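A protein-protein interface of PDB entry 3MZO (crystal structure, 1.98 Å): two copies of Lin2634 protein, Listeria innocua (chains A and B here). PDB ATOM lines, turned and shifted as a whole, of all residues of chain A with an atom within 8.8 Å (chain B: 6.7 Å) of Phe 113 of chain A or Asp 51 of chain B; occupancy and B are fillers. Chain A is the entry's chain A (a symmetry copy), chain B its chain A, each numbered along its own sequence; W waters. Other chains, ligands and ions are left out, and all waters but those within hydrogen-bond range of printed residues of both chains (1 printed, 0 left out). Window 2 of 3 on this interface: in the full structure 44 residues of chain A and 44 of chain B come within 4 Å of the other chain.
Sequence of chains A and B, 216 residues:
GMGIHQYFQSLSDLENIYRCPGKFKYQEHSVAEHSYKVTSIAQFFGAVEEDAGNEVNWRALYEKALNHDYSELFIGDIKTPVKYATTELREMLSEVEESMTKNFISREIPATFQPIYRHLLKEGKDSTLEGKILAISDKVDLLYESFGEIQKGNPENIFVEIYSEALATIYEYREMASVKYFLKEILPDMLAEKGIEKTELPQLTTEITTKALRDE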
ATOM      1  N   MET A   2      15.147 -25.449   8.159  1.00  0.00           N
ATOM      2  CA  MET A   2      13.799 -24.854   8.200  1.00  0.00           C
ATOM      3  C   MET A   2      13.111 -24.952   9.579  1.00  0.00           C
ATOM      4  O   MET A   2      12.897 -26.034  10.095  1.00  0.00           O
ATOM      5  CB  MET A   2      12.923 -25.556   7.149  1.00  0.00           C
ATOM      6  CG  MET A   2      11.538 -24.937   6.880  1.00  0.00           C
ATOM      7  SD  MET A   2      10.701 -25.523   5.130  1.00  0.00           S
ATOM      8  CE  MET A   2      12.243 -25.271   3.949  1.00  0.00           C
ATOM      9  N   GLY A   3      12.780 -23.820  10.177  1.00  0.00           N
ATOM     10  CA  GLY A   3      12.004 -23.823  11.417  1.00  0.00           C
ATOM     11  C   GLY A   3      11.887 -22.442  12.033  1.00  0.00           C
ATOM     12  O   GLY A   3      12.724 -21.568  11.796  1.00  0.00           O
ATOM     13  N   ILE A   4      10.843 -22.249  12.839  1.00  0.00           N
ATOM     14  CA  ILE A   4      10.620 -21.016  13.546  1.00  0.00           C
ATOM     15  C   ILE A   4      11.756 -20.725  14.538  1.00  0.00           C
ATOM     16  O   ILE A   4      12.078 -19.564  14.787  1.00  0.00           O
ATOM     17  CB  ILE A   4       9.241 -20.993  14.252  1.00  0.00           C
ATOM     18  CG1 ILE A   4       8.108 -21.176  13.216  1.00  0.00           C
ATOM     19  CG2 ILE A   4       8.998 -19.659  14.984  1.00  0.00           C
ATOM     20  CD1 ILE A   4       7.994 -20.016  12.229  1.00  0.00           C
ATOM     21  N   TYR A   7      14.111 -18.564  12.839  1.00  0.00           N
ATOM     22  CA  TYR A   7      13.563 -17.217  12.743  1.00  0.00           C
ATOM     23  C   TYR A   7      13.747 -16.469  14.069  1.00  0.00           C
ATOM     24  O   TYR A   7      14.191 -15.312  14.077  1.00  0.00           O
ATOM     25  CB  TYR A   7      12.107 -17.269  12.345  1.00  0.00           C
ATOM     26  CG  TYR A   7      11.399 -15.965  12.534  1.00  0.00           C
ATOM     27  CD1 TYR A   7      11.657 -14.883  11.704  1.00  0.00           C
ATOM     28  CD2 TYR A   7      10.458 -15.813  13.525  1.00  0.00           C
ATOM     29  CE1 TYR A   7      11.008 -13.665  11.878  1.00  0.00           C
ATOM     30  CE2 TYR A   7       9.839 -14.585  13.747  1.00  0.00           C
ATOM     31  CZ  TYR A   7      10.115 -13.510  12.914  1.00  0.00           C
ATOM     32  OH  TYR A   7       9.448 -12.318  13.111  1.00  0.00           O
ATOM     33  N   ARG A  59      -3.910  -4.392  13.530  1.00  0.00           N
ATOM     34  CA  ARG A  59      -3.003  -5.431  13.110  1.00  0.00           C
ATOM     35  C   ARG A  59      -2.125  -4.963  11.947  1.00  0.00           C
ATOM     36  O   ARG A  59      -0.905  -5.188  11.934  1.00  0.00           O
ATOM     37  CB  ARG A  59      -3.738  -6.703  12.728  1.00  0.00           C
ATOM     38  CG  ARG A  59      -2.784  -7.858  12.516  1.00  0.00           C
ATOM     39  CD  ARG A  59      -3.539  -9.145  12.163  1.00  0.00           C
ATOM     40  NE  ARG A  59      -2.633 -10.297  12.094  1.00  0.00           N
ATOM     41  CZ  ARG A  59      -3.018 -11.535  11.794  1.00  0.00           C
ATOM     42  NH1 ARG A  59      -4.293 -11.788  11.543  1.00  0.00           N
ATOM     43  NH2 ARG A  59      -2.131 -12.530  11.777  1.00  0.00           N
ATOM     44  N   ILE A 105      12.261 -17.018   2.960  1.00  0.00           N
ATOM     45  CA  ILE A 105      11.011 -17.661   3.417  1.00  0.00           C
ATOM     46  C   ILE A 105      10.915 -19.126   2.993  1.00  0.00           C
ATOM     47  O   ILE A 105      10.434 -19.979   3.760  1.00  0.00           O
ATOM     48  CB  ILE A 105       9.775 -16.866   2.904  1.00  0.00           C
ATOM     49  CG1 ILE A 105       9.661 -15.531   3.655  1.00  0.00           C
ATOM     50  CG2 ILE A 105       8.491 -17.699   3.030  1.00  0.00           C
ATOM     51  CD1 ILE A 105       8.630 -14.539   3.061  1.00  0.00           C
ATOM     52  N   SER A 106      11.334 -19.399   1.763  1.00  0.00           N
ATOM     53  CA  SER A 106      11.307 -20.746   1.179  1.00  0.00           C
ATOM     54  C   SER A 106      12.276 -21.684   1.894  1.00  0.00           C
ATOM     55  O   SER A 106      11.982 -22.863   2.098  1.00  0.00           O
ATOM     56  CB  SER A 106      11.710 -20.689  -0.300  1.00  0.00           C
ATOM     57  OG  SER A 106      10.678 -20.126  -1.090  1.00  0.00           O
ATOM     58  N   GLU A 108      13.852 -21.046   5.086  1.00  0.00           N
ATOM     59  CA  GLU A 108      13.909 -21.002   6.536  1.00  0.00           C
ATOM     60  C   GLU A 108      12.564 -21.165   7.254  1.00  0.00           C
ATOM     61  O   GLU A 108      12.547 -21.613   8.397  1.00  0.00           O
ATOM     62  CB  GLU A 108      14.499 -19.663   6.947  1.00  0.00           C
ATOM     63  CG  GLU A 108      15.778 -19.284   6.220  1.00  0.00           C
ATOM     64  CD  GLU A 108      16.989 -20.043   6.694  1.00  0.00           C
ATOM     65  OE1 GLU A 108      16.937 -20.673   7.786  1.00  0.00           O
ATOM     66  OE2 GLU A 108      18.008 -19.981   5.966  1.00  0.00           O
ATOM     67  N   ILE A 109      11.447 -20.768   6.619  1.00  0.00           N
ATOM     68  CA  ILE A 109      10.128 -20.800   7.294  1.00  0.00           C
ATOM     69  C   ILE A 109       9.368 -22.093   6.928  1.00  0.00           C
ATOM     70  O   ILE A 109       9.296 -22.471   5.750  1.00  0.00           O
ATOM     71  CB  ILE A 109       9.263 -19.528   6.984  1.00  0.00           C
ATOM     72  CG1 ILE A 109      10.020 -18.244   7.319  1.00  0.00           C
ATOM     73  CG2 ILE A 109       7.911 -19.552   7.733  1.00  0.00           C
ATOM     74  CD1 ILE A 109      10.435 -18.090   8.811  1.00  0.00           C
ATOM     75  N   PRO A 110       8.808 -22.798   7.935  1.00  0.00           N
ATOM     76  CA  PRO A 110       7.995 -23.966   7.601  1.00  0.00           C
ATOM     77  C   PRO A 110       6.832 -23.600   6.641  1.00  0.00           C
ATOM     78  O   PRO A 110       6.280 -22.498   6.752  1.00  0.00           O
ATOM     79  CB  PRO A 110       7.452 -24.389   8.971  1.00  0.00           C
ATOM     80  CG  PRO A 110       8.503 -23.955   9.907  1.00  0.00           C
ATOM     81  CD  PRO A 110       8.863 -22.609   9.398  1.00  0.00           C
ATOM     82  N   ALA A 111       6.470 -24.513   5.733  1.00  0.00           N
ATOM     83  CA  ALA A 111       5.361 -24.263   4.787  1.00  0.00           C
ATOM     84  C   ALA A 111       4.104 -23.711   5.478  1.00  0.00           C
ATOM     85  O   ALA A 111       3.522 -22.737   5.008  1.00  0.00           O
ATOM     86  CB  ALA A 111       5.032 -25.517   3.954  1.00  0.00           C
ATOM     87  N   THR A 112       3.691 -24.296   6.594  1.00  0.00           N
ATOM     88  CA  THR A 112       2.505 -23.798   7.292  1.00  0.00           C
ATOM     89  C   THR A 112       2.533 -22.293   7.533  1.00  0.00           C
ATOM     90  O   THR A 112       1.490 -21.657   7.452  1.00  0.00           O
ATOM     91  CB  THR A 112       2.272 -24.499   8.648  1.00  0.00           C
ATOM     92  OG1 THR A 112       2.146 -25.888   8.414  1.00  0.00           O
ATOM     93  CG2 THR A 112       1.000 -24.008   9.323  1.00  0.00           C
ATOM     94  N   PHE A 113       3.711 -21.717   7.810  1.00  0.00           N
ATOM     95  CA  PHE A 113       3.782 -20.281   8.153  1.00  0.00           C
ATOM     96  C   PHE A 113       4.333 -19.385   7.052  1.00  0.00           C
ATOM     97  O   PHE A 113       4.451 -18.184   7.234  1.00  0.00           O
ATOM     98  CB  PHE A 113       4.599 -20.098   9.452  1.00  0.00           C
ATOM     99  CG  PHE A 113       3.931 -20.743  10.647  1.00  0.00           C
ATOM    100  CD1 PHE A 113       2.760 -20.192  11.182  1.00  0.00           C
ATOM    101  CD2 PHE A 113       4.408 -21.933  11.166  1.00  0.00           C
ATOM    102  CE1 PHE A 113       2.109 -20.802  12.239  1.00  0.00           C
ATOM    103  CE2 PHE A 113       3.775 -22.537  12.246  1.00  0.00           C
ATOM    104  CZ  PHE A 113       2.616 -21.976  12.775  1.00  0.00           C
ATOM    105  N   GLN A 114       4.708 -19.976   5.918  1.00  0.00           N
ATOM    106  CA  GLN A 114       5.216 -19.175   4.799  1.00  0.00           C
ATOM    107  C   GLN A 114       4.217 -18.069   4.367  1.00  0.00           C
ATOM    108  O   GLN A 114       4.641 -16.936   4.123  1.00  0.00           O
ATOM    109  CB  GLN A 114       5.654 -20.068   3.628  1.00  0.00           C
ATOM    110  CG  GLN A 114       6.928 -20.918   3.958  1.00  0.00           C
ATOM    111  CD  GLN A 114       7.444 -21.737   2.784  1.00  0.00           C
ATOM    112  OE1 GLN A 114       6.926 -21.624   1.692  1.00  0.00           O
ATOM    113  NE2 GLN A 114       8.453 -22.586   3.020  1.00  0.00           N
ATOM    114  N   PRO A 115       2.913 -18.381   4.304  1.00  0.00           N
ATOM    115  CA  PRO A 115       1.952 -17.361   3.855  1.00  0.00           C
ATOM    116  C   PRO A 115       1.892 -16.161   4.781  1.00  0.00           C
ATOM    117  O   PRO A 115       1.867 -15.016   4.291  1.00  0.00           O
ATOM    118  CB  PRO A 115       0.625 -18.107   3.847  1.00  0.00           C
ATOM    119  CG  PRO A 115       1.008 -19.477   3.491  1.00  0.00           C
ATOM    120  CD  PRO A 115       2.251 -19.697   4.367  1.00  0.00           C
ATOM    121  N   ILE A 116       1.879 -16.401   6.089  1.00  0.00           N
ATOM    122  CA  ILE A 116       1.872 -15.265   7.032  1.00  0.00           C
ATOM    123  C   ILE A 116       3.176 -14.452   6.965  1.00  0.00           C
ATOM    124  O   ILE A 116       3.109 -13.226   6.937  1.00  0.00           O
ATOM    125  CB  ILE A 116       1.450 -15.641   8.504  1.00  0.00           C
ATOM    126  CG1 ILE A 116       1.249 -14.355   9.329  1.00  0.00           C
ATOM    127  CG2 ILE A 116       2.451 -16.572   9.148  1.00  0.00           C
ATOM    128  CD1 ILE A 116       0.232 -13.287   8.704  1.00  0.00           C
ATOM    129  N   TYR A 117       4.340 -15.109   6.858  1.00  0.00           N
ATOM    130  CA  TYR A 117       5.617 -14.388   6.650  1.00  0.00           C
ATOM    131  C   TYR A 117       5.773 -13.673   5.317  1.00  0.00           C
ATOM    132  O   TYR A 117       6.424 -12.620   5.247  1.00  0.00           O
ATOM    133  CB  TYR A 117       6.851 -15.288   6.957  1.00  0.00           C
ATOM    134  CG  TYR A 117       6.930 -15.373   8.446  1.00  0.00           C
ATOM    135  CD1 TYR A 117       6.279 -16.395   9.144  1.00  0.00           C
ATOM    136  CD2 TYR A 117       7.484 -14.320   9.176  1.00  0.00           C
ATOM    137  CE1 TYR A 117       6.247 -16.394  10.572  1.00  0.00           C
ATOM    138  CE2 TYR A 117       7.463 -14.314  10.582  1.00  0.00           C
ATOM    139  CZ  TYR A 117       6.845 -15.351  11.267  1.00  0.00           C
ATOM    140  OH  TYR A 117       6.828 -15.311  12.645  1.00  0.00           O
ATOM    141  N   ARG A 118       5.173 -14.226   4.269  1.00  0.00           N
ATOM    142  CA  ARG A 118       5.133 -13.574   2.955  1.00  0.00           C
ATOM    143  C   ARG A 118       4.365 -12.239   3.118  1.00  0.00           C
ATOM    144  O   ARG A 118       4.798 -11.149   2.632  1.00  0.00           O
ATOM    145  CB  ARG A 118       4.444 -14.528   1.951  1.00  0.00           C
ATOM    146  CG  ARG A 118       4.867 -14.437   0.532  1.00  0.00           C
ATOM    147  CD  ARG A 118       4.358 -15.643  -0.278  1.00  0.00           C
ATOM    148  NE  ARG A 118       5.294 -16.764  -0.208  1.00  0.00           N
ATOM    149  CZ  ARG A 118       5.035 -18.002   0.230  1.00  0.00           C
ATOM    150  NH1 ARG A 118       3.825 -18.351   0.657  1.00  0.00           N
ATOM    151  NH2 ARG A 118       6.013 -18.919   0.214  1.00  0.00           N
ATOM    152  N   HIS A 119       3.248 -12.316   3.827  1.00  0.00           N
ATOM    153  CA  HIS A 119       2.452 -11.134   4.145  1.00  0.00           C
ATOM    154  C   HIS A 119       3.174 -10.118   5.057  1.00  0.00           C
ATOM    155  O   HIS A 119       3.115  -8.899   4.829  1.00  0.00           O
ATOM    156  CB  HIS A 119       1.133 -11.509   4.836  1.00  0.00           C
ATOM    157  CG  HIS A 119       0.338 -10.310   5.243  1.00  0.00           C
ATOM    158  ND1 HIS A 119      -0.208  -9.447   4.317  1.00  0.00           N
ATOM    159  CD2 HIS A 119       0.068  -9.779   6.460  1.00  0.00           C
ATOM    160  CE1 HIS A 119      -0.814  -8.459   4.947  1.00  0.00           C
ATOM    161  NE2 HIS A 119      -0.667  -8.638   6.249  1.00  0.00           N
ATOM    162  N   LEU A 120       3.815 -10.617   6.110  1.00  0.00           N
ATOM    163  CA  LEU A 120       4.480  -9.739   7.087  1.00  0.00           C
ATOM    164  C   LEU A 120       5.724  -9.042   6.523  1.00  0.00           C
ATOM    165  O   LEU A 120       6.050  -7.946   6.956  1.00  0.00           O
ATOM    166  CB  LEU A 120       4.867 -10.533   8.346  1.00  0.00           C
ATOM    167  CG  LEU A 120       3.741 -11.100   9.248  1.00  0.00           C
ATOM    168  CD1 LEU A 120       4.320 -12.081  10.291  1.00  0.00           C
ATOM    169  CD2 LEU A 120       2.961  -9.995   9.954  1.00  0.00           C
ATOM    170  N   LEU A 121       6.420  -9.677   5.579  1.00  0.00           N
ATOM    171  CA  LEU A 121       7.706  -9.176   5.116  1.00  0.00           C
ATOM    172  C   LEU A 121       7.632  -8.479   3.777  1.00  0.00           C
ATOM    173  O   LEU A 121       8.648  -8.062   3.258  1.00  0.00           O
ATOM    174  CB  LEU A 121       8.703 -10.331   5.028  1.00  0.00           C
ATOM    175  CG  LEU A 121       8.989 -11.012   6.357  1.00  0.00           C
ATOM    176  CD1 LEU A 121      10.137 -11.964   6.120  1.00  0.00           C
ATOM    177  CD2 LEU A 121       9.311  -9.990   7.498  1.00  0.00           C
ATOM    178  N   PHE B  44       4.180 -13.845  16.204  1.00  0.00           N
ATOM    179  CA  PHE B  44       4.135 -15.235  15.766  1.00  0.00           C
ATOM    180  C   PHE B  44       3.076 -16.048  16.546  1.00  0.00           C
ATOM    181  O   PHE B  44       2.259 -16.745  15.965  1.00  0.00           O
ATOM    182  CB  PHE B  44       5.480 -15.925  15.879  1.00  0.00           C
ATOM    183  CG  PHE B  44       5.406 -17.414  15.646  1.00  0.00           C
ATOM    184  CD1 PHE B  44       5.248 -17.912  14.369  1.00  0.00           C
ATOM    185  CD2 PHE B  44       5.425 -18.307  16.703  1.00  0.00           C
ATOM    186  CE1 PHE B  44       5.124 -19.253  14.148  1.00  0.00           C
ATOM    187  CE2 PHE B  44       5.302 -19.673  16.472  1.00  0.00           C
ATOM    188  CZ  PHE B  44       5.155 -20.138  15.177  1.00  0.00           C
ATOM    189  N   GLY B  46       0.455 -15.102  18.064  1.00  0.00           N
ATOM    190  CA  GLY B  46      -0.854 -14.648  17.662  1.00  0.00           C
ATOM    191  C   GLY B  46      -1.334 -15.418  16.467  1.00  0.00           C
ATOM    192  O   GLY B  46      -2.483 -15.857  16.434  1.00  0.00           O
ATOM    193  N   ALA B  47      -0.451 -15.595  15.487  1.00  0.00           N
ATOM    194  CA  ALA B  47      -0.793 -16.349  14.265  1.00  0.00           C
ATOM    195  C   ALA B  47      -1.125 -17.799  14.569  1.00  0.00           C
ATOM    196  O   ALA B  47      -2.049 -18.364  13.960  1.00  0.00           O
ATOM    197  CB  ALA B  47       0.351 -16.286  13.236  1.00  0.00           C
ATOM    198  N   VAL B  48      -0.350 -18.402  15.471  1.00  0.00           N
ATOM    199  CA  VAL B  48      -0.579 -19.782  15.924  1.00  0.00           C
ATOM    200  C   VAL B  48      -1.994 -19.892  16.567  1.00  0.00           C
ATOM    201  O   VAL B  48      -2.754 -20.835  16.300  1.00  0.00           O
ATOM    202  CB  VAL B  48       0.502 -20.229  16.950  1.00  0.00           C
ATOM    203  CG1 VAL B  48       0.160 -21.603  17.574  1.00  0.00           C
ATOM    204  CG2 VAL B  48       1.893 -20.276  16.305  1.00  0.00           C
ATOM    205  N   GLU B  49      -2.334 -18.933  17.423  1.00  0.00           N
ATOM    206  CA  GLU B  49      -3.622 -18.975  18.118  1.00  0.00           C
ATOM    207  C   GLU B  49      -4.798 -18.827  17.123  1.00  0.00           C
ATOM    208  O   GLU B  49      -5.824 -19.497  17.251  1.00  0.00           O
ATOM    209  CB  GLU B  49      -3.678 -17.906  19.202  1.00  0.00           C
ATOM    210  CG  GLU B  49      -2.694 -18.118  20.350  1.00  0.00           C
ATOM    211  CD  GLU B  49      -2.985 -19.349  21.194  1.00  0.00           C
ATOM    212  OE1 GLU B  49      -4.141 -19.804  21.176  1.00  0.00           O
ATOM    213  OE2 GLU B  49      -2.055 -19.856  21.867  1.00  0.00           O
ATOM    214  N   GLU B  50      -4.639 -17.972  16.113  1.00  0.00           N
ATOM    215  CA  GLU B  50      -5.682 -17.802  15.099  1.00  0.00           C
ATOM    216  C   GLU B  50      -5.821 -19.058  14.255  1.00  0.00           C
ATOM    217  O   GLU B  50      -6.941 -19.440  13.946  1.00  0.00           O
ATOM    218  CB  GLU B  50      -5.446 -16.587  14.204  1.00  0.00           C
ATOM    219  CG  GLU B  50      -5.822 -15.310  14.881  1.00  0.00           C
ATOM    220  CD  GLU B  50      -6.133 -14.184  13.910  1.00  0.00           C
ATOM    221  OE1 GLU B  50      -5.572 -14.174  12.785  1.00  0.00           O
ATOM    222  OE2 GLU B  50      -6.916 -13.303  14.296  1.00  0.00           O
ATOM    223  N   ASP B  51      -4.697 -19.679  13.881  1.00  0.00           N
ATOM    224  CA  ASP B  51      -4.712 -20.952  13.163  1.00  0.00           C
ATOM    225  C   ASP B  51      -5.485 -22.002  14.007  1.00  0.00           C
ATOM    226  O   ASP B  51      -6.163 -22.875  13.445  1.00  0.00           O
ATOM    227  CB  ASP B  51      -3.282 -21.495  12.856  1.00  0.00           C
ATOM    228  CG  ASP B  51      -2.592 -20.862  11.562  1.00  0.00           C
ATOM    229  OD1 ASP B  51      -3.240 -20.146  10.770  1.00  0.00           O
ATOM    230  OD2 ASP B  51      -1.363 -21.105  11.318  1.00  0.00           O
ATOM    231  N   ALA B  52      -5.373 -21.930  15.334  1.00  0.00           N
ATOM    232  CA  ALA B  52      -6.033 -22.898  16.216  1.00  0.00           C
ATOM    233  C   ALA B  52      -7.503 -22.564  16.435  1.00  0.00           C
ATOM    234  O   ALA B  52      -8.179 -23.269  17.172  1.00  0.00           O
ATOM    235  CB  ALA B  52      -5.331 -22.974  17.562  1.00  0.00           C
ATOM    236  N   GLY B  53      -7.990 -21.468  15.849  1.00  0.00           N
ATOM    237  CA  GLY B  53      -9.385 -21.090  15.967  1.00  0.00           C
ATOM    238  C   GLY B  53      -9.686 -20.044  17.011  1.00  0.00           C
ATOM    239  O   GLY B  53     -10.841 -19.716  17.222  1.00  0.00           O
ATOM    240  N   ASN B  54      -8.664 -19.464  17.635  1.00  0.00           N
ATOM    241  CA  ASN B  54      -8.890 -18.482  18.690  1.00  0.00           C
ATOM    242  C   ASN B  54      -8.850 -17.057  18.192  1.00  0.00           C
ATOM    243  O   ASN B  54      -7.913 -16.638  17.509  1.00  0.00           O
ATOM    244  CB  ASN B  54      -7.896 -18.690  19.835  1.00  0.00           C
ATOM    245  CG  ASN B  54      -7.981 -20.091  20.412  1.00  0.00           C
ATOM    246  OD1 ASN B  54      -9.065 -20.525  20.791  1.00  0.00           O
ATOM    247  ND2 ASN B  54      -6.858 -20.821  20.445  1.00  0.00           N
ATOM    248  N   TYR B 181       2.796 -25.704  20.321  1.00  0.00           N
ATOM    249  CA  TYR B 181       3.647 -25.576  19.153  1.00  0.00           C
ATOM    250  C   TYR B 181       5.130 -25.396  19.537  1.00  0.00           C
ATOM    251  O   TYR B 181       6.020 -26.031  18.969  1.00  0.00           O
ATOM    252  CB  TYR B 181       3.177 -24.404  18.267  1.00  0.00           C
ATOM    253  CG  TYR B 181       3.950 -24.390  17.025  1.00  0.00           C
ATOM    254  CD1 TYR B 181       3.611 -25.226  15.976  1.00  0.00           C
ATOM    255  CD2 TYR B 181       5.100 -23.633  16.924  1.00  0.00           C
ATOM    256  CE1 TYR B 181       4.387 -25.275  14.832  1.00  0.00           C
ATOM    257  CE2 TYR B 181       5.867 -23.661  15.777  1.00  0.00           C
ATOM    258  CZ  TYR B 181       5.507 -24.492  14.746  1.00  0.00           C
ATOM    259  OH  TYR B 181       6.274 -24.546  13.629  1.00  0.00           O
HETATM  260  O   HOH W   1       9.103 -24.654  13.649  1.00  0.00           O
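Printed residues of chain A that touch a printed residue of chain B: Ile 4, Arg 59, Phe 113 and Tyr 117. Of the 11 printed residues of chain B, 5 touch a printed residue of chain A. Hydrophobic or aromatic side chains of chain B within 4 Å of the printed part of chain A: Phe 44, Val 48 and Tyr 181.
Among the printed residues, merely in contact across the chains: Phe 113 of chain A with Tyr 181 of chain B (3.5 Å), Tyr 117 of chain A with Phe 44 of chain B (3.5 Å), Ile 4 of chain A with Phe 44 of chain B (3.5 Å), Phe 113 of chain A with Asp 51 of chain B (3.6 Å), Ile 4 of chain A with Tyr 181 of chain B (3.9 Å), Phe 113 of chain A with Phe 44 of chain B (3.9 Å) and Phe 113 of chain A with Val 48 of chain B (3.98 Å).
No position is printed for both chains. Of the 8 pairs that touch across the chains among the printed residues, none has its exchanged pair printed and touching as well.
Printed residues of chain B within 4 Å of Phe 113 of chain A: Phe 44, Val 48, Asp 51 and Tyr 181. Asp 51 of chain B touches one residue of chain A. Of the printed residues of chain A, Glu 50 of chain B touches Arg 59 (3.0 Å). Of the printed residues of chain B, Tyr 117 of chain A touches Phe 44 (3.5 Å). Printed residues of chain A within 4 Å of Phe 44 of chain B: Ile 4, Phe 113 and Tyr 117. Printed residues of chain A within 4 Å of Val 48 of chain B: Phe 113. Ala 47 of chain B touches none of the printed residues of chain A. Gln 114 of chain A touches none of the printed residues of chain B. The nearest printed residue of chain B that does not touch Phe 113 of chain A is Ala 47 of chain B (4.9 Å). The nearest printed residue of chain B that does not touch Ile 4 of chain A is Val 48 of chain B (7.0 Å).
The guanidinium group of Arg 59 of chain A is in salt-bridge range of the side-chain carboxylate of Glu 50 of chain B (3.0 Å).
Water W1 bridges OH of Tyr 181 of chain B (2.8 Å) and N of Ile 4 of chain A (3.1 Å).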
